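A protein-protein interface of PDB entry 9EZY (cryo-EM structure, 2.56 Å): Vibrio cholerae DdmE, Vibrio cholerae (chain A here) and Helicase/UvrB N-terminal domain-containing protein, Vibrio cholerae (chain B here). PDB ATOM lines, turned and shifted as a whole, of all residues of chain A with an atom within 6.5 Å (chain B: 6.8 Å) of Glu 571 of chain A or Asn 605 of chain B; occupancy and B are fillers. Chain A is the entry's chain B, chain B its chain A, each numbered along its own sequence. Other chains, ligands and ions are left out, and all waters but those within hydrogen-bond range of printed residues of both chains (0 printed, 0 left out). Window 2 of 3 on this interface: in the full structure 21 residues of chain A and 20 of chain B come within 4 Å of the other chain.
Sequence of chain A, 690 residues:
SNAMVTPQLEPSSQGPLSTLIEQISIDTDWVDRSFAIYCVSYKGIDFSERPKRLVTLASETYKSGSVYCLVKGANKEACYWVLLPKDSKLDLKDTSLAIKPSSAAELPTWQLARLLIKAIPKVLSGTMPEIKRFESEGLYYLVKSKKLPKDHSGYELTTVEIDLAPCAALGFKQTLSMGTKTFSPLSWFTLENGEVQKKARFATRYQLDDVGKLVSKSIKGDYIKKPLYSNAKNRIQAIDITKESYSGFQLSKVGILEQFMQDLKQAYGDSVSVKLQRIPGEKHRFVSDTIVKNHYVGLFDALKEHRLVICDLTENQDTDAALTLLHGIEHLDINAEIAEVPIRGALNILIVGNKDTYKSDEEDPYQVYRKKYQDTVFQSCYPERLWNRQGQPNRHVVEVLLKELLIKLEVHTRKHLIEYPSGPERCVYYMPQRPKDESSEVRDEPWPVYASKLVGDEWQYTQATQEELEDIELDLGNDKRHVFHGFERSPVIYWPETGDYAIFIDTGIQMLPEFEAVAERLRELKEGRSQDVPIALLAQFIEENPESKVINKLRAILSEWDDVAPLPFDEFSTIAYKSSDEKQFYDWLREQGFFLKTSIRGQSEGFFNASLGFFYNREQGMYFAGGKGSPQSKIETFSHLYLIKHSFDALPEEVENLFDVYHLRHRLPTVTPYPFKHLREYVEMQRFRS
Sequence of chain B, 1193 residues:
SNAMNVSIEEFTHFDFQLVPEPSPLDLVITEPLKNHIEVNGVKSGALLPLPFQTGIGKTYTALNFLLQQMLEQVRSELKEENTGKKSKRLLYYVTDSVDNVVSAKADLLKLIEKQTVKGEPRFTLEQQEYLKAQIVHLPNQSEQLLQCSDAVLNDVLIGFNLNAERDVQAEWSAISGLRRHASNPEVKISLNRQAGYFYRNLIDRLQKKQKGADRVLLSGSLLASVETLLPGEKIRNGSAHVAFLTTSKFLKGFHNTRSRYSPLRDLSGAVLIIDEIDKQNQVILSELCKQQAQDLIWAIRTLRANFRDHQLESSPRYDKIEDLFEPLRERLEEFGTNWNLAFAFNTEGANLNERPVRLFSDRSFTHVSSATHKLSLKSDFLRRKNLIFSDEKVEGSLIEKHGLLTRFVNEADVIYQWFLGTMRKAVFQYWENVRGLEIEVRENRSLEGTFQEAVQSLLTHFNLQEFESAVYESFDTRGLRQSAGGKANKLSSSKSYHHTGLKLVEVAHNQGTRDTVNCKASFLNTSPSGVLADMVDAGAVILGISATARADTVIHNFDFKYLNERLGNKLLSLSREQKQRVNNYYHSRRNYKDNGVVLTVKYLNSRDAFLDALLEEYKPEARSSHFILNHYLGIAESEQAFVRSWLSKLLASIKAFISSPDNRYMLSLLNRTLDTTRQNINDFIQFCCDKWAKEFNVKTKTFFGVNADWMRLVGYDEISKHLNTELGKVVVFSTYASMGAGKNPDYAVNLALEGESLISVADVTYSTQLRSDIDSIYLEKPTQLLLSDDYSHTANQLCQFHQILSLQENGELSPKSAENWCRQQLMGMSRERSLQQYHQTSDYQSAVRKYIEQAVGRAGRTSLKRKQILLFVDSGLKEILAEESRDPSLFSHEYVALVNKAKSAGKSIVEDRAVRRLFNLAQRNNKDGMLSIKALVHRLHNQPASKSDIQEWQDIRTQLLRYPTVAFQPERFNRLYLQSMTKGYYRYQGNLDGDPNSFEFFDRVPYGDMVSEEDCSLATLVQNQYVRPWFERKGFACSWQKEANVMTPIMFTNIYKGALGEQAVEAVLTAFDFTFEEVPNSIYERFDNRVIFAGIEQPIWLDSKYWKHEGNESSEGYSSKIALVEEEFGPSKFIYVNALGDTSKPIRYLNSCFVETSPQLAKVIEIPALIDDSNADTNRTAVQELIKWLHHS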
ATOM      1  N   ILE A 557     -14.345   6.574  -2.755  1.00  0.00           N
ATOM      2  CA  ILE A 557     -13.719   6.501  -4.073  1.00  0.00           C
ATOM      3  C   ILE A 557     -12.205   6.623  -3.948  1.00  0.00           C
ATOM      4  O   ILE A 557     -11.449   5.867  -4.569  1.00  0.00           O
ATOM      5  CB  ILE A 557     -14.299   7.581  -5.004  1.00  0.00           C
ATOM      6  CG1 ILE A 557     -15.739   7.233  -5.385  1.00  0.00           C
ATOM      7  CG2 ILE A 557     -13.444   7.722  -6.249  1.00  0.00           C
ATOM      8  CD1 ILE A 557     -16.533   8.409  -5.907  1.00  0.00           C
ATOM      9  N   GLU A 560     -10.505   3.584  -2.622  1.00  0.00           N
ATOM     10  CA  GLU A 560     -10.437   2.550  -3.645  1.00  0.00           C
ATOM     11  C   GLU A 560      -9.648   3.003  -4.867  1.00  0.00           C
ATOM     12  O   GLU A 560      -9.949   2.577  -5.986  1.00  0.00           O
ATOM     13  CB  GLU A 560     -11.847   2.129  -4.056  1.00  0.00           C
ATOM     14  CG  GLU A 560     -12.688   1.590  -2.913  1.00  0.00           C
ATOM     15  CD  GLU A 560     -13.985   0.966  -3.387  1.00  0.00           C
ATOM     16  OE1 GLU A 560     -14.585   1.496  -4.347  1.00  0.00           O
ATOM     17  OE2 GLU A 560     -14.407  -0.053  -2.800  1.00  0.00           O
ATOM     18  N   TRP A 561      -8.650   3.862  -4.675  1.00  0.00           N
ATOM     19  CA  TRP A 561      -7.881   4.439  -5.766  1.00  0.00           C
ATOM     20  C   TRP A 561      -6.440   4.641  -5.310  1.00  0.00           C
ATOM     21  O   TRP A 561      -6.139   4.666  -4.113  1.00  0.00           O
ATOM     22  CB  TRP A 561      -8.508   5.761  -6.230  1.00  0.00           C
ATOM     23  CG  TRP A 561      -7.804   6.390  -7.385  1.00  0.00           C
ATOM     24  CD1 TRP A 561      -6.970   7.463  -7.345  1.00  0.00           C
ATOM     25  CD2 TRP A 561      -7.870   5.984  -8.757  1.00  0.00           C
ATOM     26  NE1 TRP A 561      -6.509   7.755  -8.604  1.00  0.00           N
ATOM     27  CE2 TRP A 561      -7.048   6.860  -9.490  1.00  0.00           C
ATOM     28  CE3 TRP A 561      -8.545   4.966  -9.435  1.00  0.00           C
ATOM     29  CZ2 TRP A 561      -6.881   6.750 -10.867  1.00  0.00           C
ATOM     30  CZ3 TRP A 561      -8.378   4.858 -10.802  1.00  0.00           C
ATOM     31  CH2 TRP A 561      -7.554   5.744 -11.504  1.00  0.00           C
ATOM     32  N   LEU A 567      -7.595  11.135 -10.602  1.00  0.00           N
ATOM     33  CA  LEU A 567      -8.810  10.373 -10.866  1.00  0.00           C
ATOM     34  C   LEU A 567      -9.401  10.772 -12.214  1.00  0.00           C
ATOM     35  O   LEU A 567      -9.659  11.958 -12.442  1.00  0.00           O
ATOM     36  CB  LEU A 567      -9.842  10.604  -9.769  1.00  0.00           C
ATOM     37  CG  LEU A 567      -9.684   9.712  -8.540  1.00  0.00           C
ATOM     38  CD1 LEU A 567      -8.552  10.226  -7.670  1.00  0.00           C
ATOM     39  CD2 LEU A 567     -10.975   9.630  -7.749  1.00  0.00           C
ATOM     40  N   PRO A 568      -9.628   9.828 -13.127  1.00  0.00           N
ATOM     41  CA  PRO A 568     -10.384  10.156 -14.339  1.00  0.00           C
ATOM     42  C   PRO A 568     -11.850  10.398 -14.018  1.00  0.00           C
ATOM     43  O   PRO A 568     -12.381   9.910 -13.018  1.00  0.00           O
ATOM     44  CB  PRO A 568     -10.198   8.921 -15.224  1.00  0.00           C
ATOM     45  CG  PRO A 568      -9.920   7.814 -14.281  1.00  0.00           C
ATOM     46  CD  PRO A 568      -9.203   8.417 -13.109  1.00  0.00           C
ATOM     47  N   PHE A 569     -12.508  11.167 -14.889  1.00  0.00           N
ATOM     48  CA  PHE A 569     -13.898  11.540 -14.640  1.00  0.00           C
ATOM     49  C   PHE A 569     -14.780  10.314 -14.446  1.00  0.00           C
ATOM     50  O   PHE A 569     -15.782  10.367 -13.725  1.00  0.00           O
ATOM     51  CB  PHE A 569     -14.436  12.384 -15.793  1.00  0.00           C
ATOM     52  CG  PHE A 569     -15.935  12.399 -15.876  1.00  0.00           C
ATOM     53  CD1 PHE A 569     -16.690  12.926 -14.843  1.00  0.00           C
ATOM     54  CD2 PHE A 569     -16.588  11.872 -16.975  1.00  0.00           C
ATOM     55  CE1 PHE A 569     -18.069  12.937 -14.909  1.00  0.00           C
ATOM     56  CE2 PHE A 569     -17.967  11.879 -17.047  1.00  0.00           C
ATOM     57  CZ  PHE A 569     -18.708  12.412 -16.013  1.00  0.00           C
ATOM     58  N   ASP A 570     -14.423   9.197 -15.081  1.00  0.00           N
ATOM     59  CA  ASP A 570     -15.268   8.011 -15.017  1.00  0.00           C
ATOM     60  C   ASP A 570     -15.432   7.500 -13.593  1.00  0.00           C
ATOM     61  O   ASP A 570     -16.376   6.748 -13.322  1.00  0.00           O
ATOM     62  CB  ASP A 570     -14.690   6.910 -15.904  1.00  0.00           C
ATOM     63  CG  ASP A 570     -14.382   7.396 -17.307  1.00  0.00           C
ATOM     64  OD1 ASP A 570     -13.314   8.011 -17.503  1.00  0.00           O
ATOM     65  OD2 ASP A 570     -15.211   7.166 -18.212  1.00  0.00           O
ATOM     66  N   GLU A 571     -14.541   7.888 -12.678  1.00  0.00           N
ATOM     67  CA  GLU A 571     -14.666   7.441 -11.295  1.00  0.00           C
ATOM     68  C   GLU A 571     -15.788   8.169 -10.566  1.00  0.00           C
ATOM     69  O   GLU A 571     -16.428   7.588  -9.684  1.00  0.00           O
ATOM     70  CB  GLU A 571     -13.339   7.640 -10.564  1.00  0.00           C
ATOM     71  CG  GLU A 571     -12.168   6.908 -11.202  1.00  0.00           C
ATOM     72  CD  GLU A 571     -12.416   5.419 -11.344  1.00  0.00           C
ATOM     73  OE1 GLU A 571     -13.085   4.841 -10.464  1.00  0.00           O
ATOM     74  OE2 GLU A 571     -11.943   4.830 -12.339  1.00  0.00           O
ATOM     75  N   PHE A 572     -16.046   9.430 -10.918  1.00  0.00           N
ATOM     76  CA  PHE A 572     -17.114  10.194 -10.283  1.00  0.00           C
ATOM     77  C   PHE A 572     -18.478   9.923 -10.898  1.00  0.00           C
ATOM     78  O   PHE A 572     -19.468  10.498 -10.434  1.00  0.00           O
ATOM     79  CB  PHE A 572     -16.848  11.703 -10.370  1.00  0.00           C
ATOM     80  CG  PHE A 572     -15.413  12.105 -10.159  1.00  0.00           C
ATOM     81  CD1 PHE A 572     -14.531  11.303  -9.454  1.00  0.00           C
ATOM     82  CD2 PHE A 572     -14.950  13.300 -10.677  1.00  0.00           C
ATOM     83  CE1 PHE A 572     -13.221  11.689  -9.276  1.00  0.00           C
ATOM     84  CE2 PHE A 572     -13.644  13.688 -10.500  1.00  0.00           C
ATOM     85  CZ  PHE A 572     -12.777  12.883  -9.798  1.00  0.00           C
ATOM     86  N   SER A 573     -18.552   9.075 -11.926  1.00  0.00           N
ATOM     87  CA  SER A 573     -19.806   8.888 -12.645  1.00  0.00           C
ATOM     88  C   SER A 573     -20.949   8.525 -11.708  1.00  0.00           C
ATOM     89  O   SER A 573     -22.092   8.942 -11.932  1.00  0.00           O
ATOM     90  CB  SER A 573     -19.633   7.806 -13.712  1.00  0.00           C
ATOM     91  OG  SER A 573     -18.854   8.282 -14.795  1.00  0.00           O
ATOM     92  N   THR A 574     -20.667   7.756 -10.655  1.00  0.00           N
ATOM     93  CA  THR A 574     -21.719   7.375  -9.718  1.00  0.00           C
ATOM     94  C   THR A 574     -22.257   8.566  -8.935  1.00  0.00           C
ATOM     95  O   THR A 574     -23.335   8.461  -8.339  1.00  0.00           O
ATOM     96  CB  THR A 574     -21.209   6.313  -8.740  1.00  0.00           C
ATOM     97  OG1 THR A 574     -22.155   6.150  -7.675  1.00  0.00           O
ATOM     98  CG2 THR A 574     -19.862   6.713  -8.150  1.00  0.00           C
ATOM     99  N   ILE A 575     -21.542   9.690  -8.920  1.00  0.00           N
ATOM    100  CA  ILE A 575     -21.979  10.883  -8.199  1.00  0.00           C
ATOM    101  C   ILE A 575     -22.850  11.693  -9.155  1.00  0.00           C
ATOM    102  O   ILE A 575     -22.350  12.508  -9.931  1.00  0.00           O
ATOM    103  CB  ILE A 575     -20.795  11.701  -7.678  1.00  0.00           C
ATOM    104  CG1 ILE A 575     -19.851  10.811  -6.868  1.00  0.00           C
ATOM    105  CG2 ILE A 575     -21.288  12.862  -6.821  1.00  0.00           C
ATOM    106  CD1 ILE A 575     -18.643  11.535  -6.316  1.00  0.00           C
ATOM    107  N   TYR B 603      -8.270  -2.730  -9.563  1.00  0.00           N
ATOM    108  CA  TYR B 603      -9.565  -2.938 -10.194  1.00  0.00           C
ATOM    109  C   TYR B 603      -9.863  -1.774 -11.129  1.00  0.00           C
ATOM    110  O   TYR B 603      -9.703  -0.609 -10.754  1.00  0.00           O
ATOM    111  CB  TYR B 603     -10.659  -3.074  -9.138  1.00  0.00           C
ATOM    112  CG  TYR B 603     -10.634  -4.403  -8.420  1.00  0.00           C
ATOM    113  CD1 TYR B 603     -11.375  -5.478  -8.886  1.00  0.00           C
ATOM    114  CD2 TYR B 603      -9.863  -4.585  -7.284  1.00  0.00           C
ATOM    115  CE1 TYR B 603     -11.352  -6.693  -8.237  1.00  0.00           C
ATOM    116  CE2 TYR B 603      -9.834  -5.797  -6.628  1.00  0.00           C
ATOM    117  CZ  TYR B 603     -10.580  -6.847  -7.110  1.00  0.00           C
ATOM    118  OH  TYR B 603     -10.555  -8.057  -6.460  1.00  0.00           O
ATOM    119  N   LEU B 604     -10.300  -2.091 -12.344  1.00  0.00           N
ATOM    120  CA  LEU B 604     -10.425  -1.113 -13.415  1.00  0.00           C
ATOM    121  C   LEU B 604     -11.883  -0.959 -13.815  1.00  0.00           C
ATOM    122  O   LEU B 604     -12.584  -1.954 -14.023  1.00  0.00           O
ATOM    123  CB  LEU B 604      -9.595  -1.536 -14.628  1.00  0.00           C
ATOM    124  CG  LEU B 604      -8.099  -1.698 -14.370  1.00  0.00           C
ATOM    125  CD1 LEU B 604      -7.436  -2.335 -15.567  1.00  0.00           C
ATOM    126  CD2 LEU B 604      -7.455  -0.363 -14.054  1.00  0.00           C
ATOM    127  N   ASN B 605     -12.330   0.287 -13.923  1.00  0.00           N
ATOM    128  CA  ASN B 605     -13.650   0.603 -14.440  1.00  0.00           C
ATOM    129  C   ASN B 605     -13.555   0.969 -15.918  1.00  0.00           C
ATOM    130  O   ASN B 605     -12.475   1.212 -16.459  1.00  0.00           O
ATOM    131  CB  ASN B 605     -14.274   1.753 -13.653  1.00  0.00           C
ATOM    132  CG  ASN B 605     -14.653   1.359 -12.243  1.00  0.00           C
ATOM    133  OD1 ASN B 605     -15.523   0.515 -12.034  1.00  0.00           O
ATOM    134  ND2 ASN B 605     -13.998   1.969 -11.263  1.00  0.00           N
ATOM    135  N   SER B 606     -14.709   1.007 -16.576  1.00  0.00           N
ATOM    136  CA  SER B 606     -14.752   1.478 -17.950  1.00  0.00           C
ATOM    137  C   SER B 606     -14.279   2.924 -18.014  1.00  0.00           C
ATOM    138  O   SER B 606     -14.701   3.769 -17.220  1.00  0.00           O
ATOM    139  CB  SER B 606     -16.170   1.360 -18.507  1.00  0.00           C
ATOM    140  OG  SER B 606     -16.204   1.680 -19.886  1.00  0.00           O
ATOM    141  N   ARG B 607     -13.394   3.208 -18.966  1.00  0.00           N
ATOM    142  CA  ARG B 607     -12.795   4.532 -19.132  1.00  0.00           C
ATOM    143  C   ARG B 607     -13.158   5.033 -20.526  1.00  0.00           C
ATOM    144  O   ARG B 607     -12.463   4.757 -21.505  1.00  0.00           O
ATOM    145  CB  ARG B 607     -11.287   4.468 -18.919  1.00  0.00           C
ATOM    146  CG  ARG B 607     -10.896   4.036 -17.515  1.00  0.00           C
ATOM    147  CD  ARG B 607      -9.652   4.756 -17.018  1.00  0.00           C
ATOM    148  NE  ARG B 607      -8.843   3.916 -16.143  1.00  0.00           N
ATOM    149  CZ  ARG B 607      -9.254   3.417 -14.984  1.00  0.00           C
ATOM    150  NH1 ARG B 607     -10.466   3.663 -14.514  1.00  0.00           N
ATOM    151  NH2 ARG B 607      -8.425   2.654 -14.277  1.00  0.00           N
ATOM    152  N   ASP B 608     -14.262   5.778 -20.608  1.00  0.00           N
ATOM    153  CA  ASP B 608     -14.781   6.190 -21.907  1.00  0.00           C
ATOM    154  C   ASP B 608     -13.936   7.296 -22.527  1.00  0.00           C
ATOM    155  O   ASP B 608     -13.669   7.271 -23.733  1.00  0.00           O
ATOM    156  CB  ASP B 608     -16.234   6.642 -21.769  1.00  0.00           C
ATOM    157  CG  ASP B 608     -17.217   5.529 -22.068  1.00  0.00           C
ATOM    158  OD1 ASP B 608     -18.284   5.816 -22.651  1.00  0.00           O
ATOM    159  OD2 ASP B 608     -16.923   4.365 -21.723  1.00  0.00           O
ATOM    160  N   SER B 645     -16.684  -0.692 -23.200  1.00  0.00           N
ATOM    161  CA  SER B 645     -16.302  -0.967 -21.821  1.00  0.00           C
ATOM    162  C   SER B 645     -15.153  -1.965 -21.742  1.00  0.00           C
ATOM    163  O   SER B 645     -14.129  -1.693 -21.099  1.00  0.00           O
ATOM    164  CB  SER B 645     -17.508  -1.486 -21.039  1.00  0.00           C
ATOM    165  OG  SER B 645     -17.746  -2.851 -21.326  1.00  0.00           O
ATOM    166  N   SER B 648     -11.886  -0.670 -23.298  1.00  0.00           N
ATOM    167  CA  SER B 648     -11.272   0.363 -22.473  1.00  0.00           C
ATOM    168  C   SER B 648     -10.584  -0.240 -21.259  1.00  0.00           C
ATOM    169  O   SER B 648      -9.476   0.173 -20.901  1.00  0.00           O
ATOM    170  CB  SER B 648     -12.325   1.381 -22.042  1.00  0.00           C
ATOM    171  OG  SER B 648     -13.346   0.763 -21.279  1.00  0.00           O
ATOM    172  N   LYS B 649     -11.222  -1.214 -20.606  1.00  0.00           N
ATOM    173  CA  LYS B 649     -10.578  -1.863 -19.466  1.00  0.00           C
ATOM    174  C   LYS B 649      -9.282  -2.548 -19.890  1.00  0.00           C
ATOM    175  O   LYS B 649      -8.242  -2.413 -19.230  1.00  0.00           O
ATOM    176  CB  LYS B 649     -11.532  -2.868 -18.823  1.00  0.00           C
ATOM    177  CG  LYS B 649     -12.660  -2.231 -18.035  1.00  0.00           C
ATOM    178  CD  LYS B 649     -13.750  -3.237 -17.720  1.00  0.00           C
ATOM    179  CE  LYS B 649     -14.929  -2.579 -17.029  1.00  0.00           C
ATOM    180  NZ  LYS B 649     -16.081  -3.508 -16.883  1.00  0.00           N
ATOM    181  N   ALA B 652      -6.594   0.082 -20.639  1.00  0.00           N
ATOM    182  CA  ALA B 652      -6.073   0.653 -19.402  1.00  0.00           C
ATOM    183  C   ALA B 652      -5.092  -0.298 -18.733  1.00  0.00           C
ATOM    184  O   ALA B 652      -4.030   0.131 -18.261  1.00  0.00           O
ATOM    185  CB  ALA B 652      -7.221   0.988 -18.452  1.00  0.00           C
ATOM    186  N   VAL B 873      -7.793  -6.172 -12.767  1.00  0.00           N
ATOM    187  CA  VAL B 873      -9.037  -6.923 -12.670  1.00  0.00           C
ATOM    188  C   VAL B 873     -10.178  -6.047 -13.156  1.00  0.00           C
ATOM    189  O   VAL B 873     -10.260  -4.869 -12.793  1.00  0.00           O
ATOM    190  CB  VAL B 873      -9.305  -7.393 -11.227  1.00  0.00           C
ATOM    191  CG1 VAL B 873     -10.302  -8.537 -11.221  1.00  0.00           C
ATOM    192  CG2 VAL B 873      -8.014  -7.800 -10.549  1.00  0.00           C
ATOM    193  N   ASP B 874     -11.049  -6.619 -13.978  1.00  0.00           N
ATOM    194  CA  ASP B 874     -12.277  -5.936 -14.356  1.00  0.00           C
ATOM    195  C   ASP B 874     -13.069  -5.598 -13.101  1.00  0.00           C
ATOM    196  O   ASP B 874     -13.241  -6.445 -12.220  1.00  0.00           O
ATOM    197  CB  ASP B 874     -13.092  -6.825 -15.293  1.00  0.00           C
ATOM    198  CG  ASP B 874     -14.394  -6.185 -15.723  1.00  0.00           C
ATOM    199  OD1 ASP B 874     -14.661  -5.033 -15.325  1.00  0.00           O
ATOM    200  OD2 ASP B 874     -15.157  -6.839 -16.465  1.00  0.00           O
ATOM    201  N   SER B 875     -13.550  -4.357 -13.017  1.00  0.00           N
ATOM    202  CA  SER B 875     -14.270  -3.929 -11.823  1.00  0.00           C
ATOM    203  C   SER B 875     -15.536  -4.740 -11.594  1.00  0.00           C
ATOM    204  O   SER B 875     -16.037  -4.780 -10.466  1.00  0.00           O
ATOM    205  CB  SER B 875     -14.618  -2.444 -11.922  1.00  0.00           C
ATOM    206  OG  SER B 875     -15.337  -2.169 -13.108  1.00  0.00           O
ATOM    207  N   GLY B 876     -16.065  -5.386 -12.634  1.00  0.00           N
ATOM    208  CA  GLY B 876     -17.217  -6.248 -12.454  1.00  0.00           C
ATOM    209  C   GLY B 876     -16.956  -7.414 -11.526  1.00  0.00           C
ATOM    210  O   GLY B 876     -17.904  -8.006 -11.003  1.00  0.00           O
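OE1 of Glu 571 of chain A sits at hydrogen-bond distance from ND2 of Asn 605 of chain B.
The backbone NH (N) of Asp 608 of chain B is in hydrogen-bond range of the side-chain carboxylate (OD2) of Asp 570 of chain A.
OE2 of Glu 571 of chain A lies within salt-bridge range of NH1 of Arg 607 of chain B (2.9 Å).
OG of Ser 606 of chain B sits at hydrogen-bond distance from OD2 of Asp 608 of chain B (3.3 Å).
OD1 of Asn 605 of chain B is in hydrogen-bond range of OG of Ser 875 of chain B, 2.9 Å away.
The side-chain hydroxyl (OG) of Ser 648 of chain B sits at hydrogen-bond distance from the backbone NH (N) of Arg 607 of chain B.
The side-chain hydroxyl (OG) of Ser 606 of chain B is in hydrogen-bond range of the side-chain hydroxyl (OG) of Ser 648 of chain B (3.3 Å).
The backbone carbonyl oxygen (O) of Asp 570 of chain A lies within hydrogen-bond range of the side-chain hydroxyl (OG) of Ser 573 of chain A (3.3 Å).
Among the printed residues, pairs that only touch across the chains: Asp 570 of chain A with Ser 606 of chain B (3.4 Å) and Asp 570 of chain A with Arg 607 of chain B (3.7 Å).
Phe 569 of chain A touches none of the printed residues of chain B.
Of the printed residues of chain B, Asp 570 of chain A touches Ser 606, Arg 607 and Asp 608.
Printed residues of chain B within 4 Å of Glu 571 of chain A: Asn 605 and Arg 607.
Tyr 603 of chain B touches none of the printed residues of chain A.
Of chain A, only Glu 571 (3.1 Å) comes within 4 Å of Asn 605 of chain B.
Of the printed residues of chain A, Ser 606 of chain B touches Asp 570.
Printed residues of chain A within 4 Å of Asp 608 of chain B: Asp 570.
Among the printed residues, Asp or Glu carboxylates within 4 Å of a Lys or Arg side-chain nitrogen of the other chain: Glu 571 of chain A with Arg 607 of chain B (2.9 Å).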
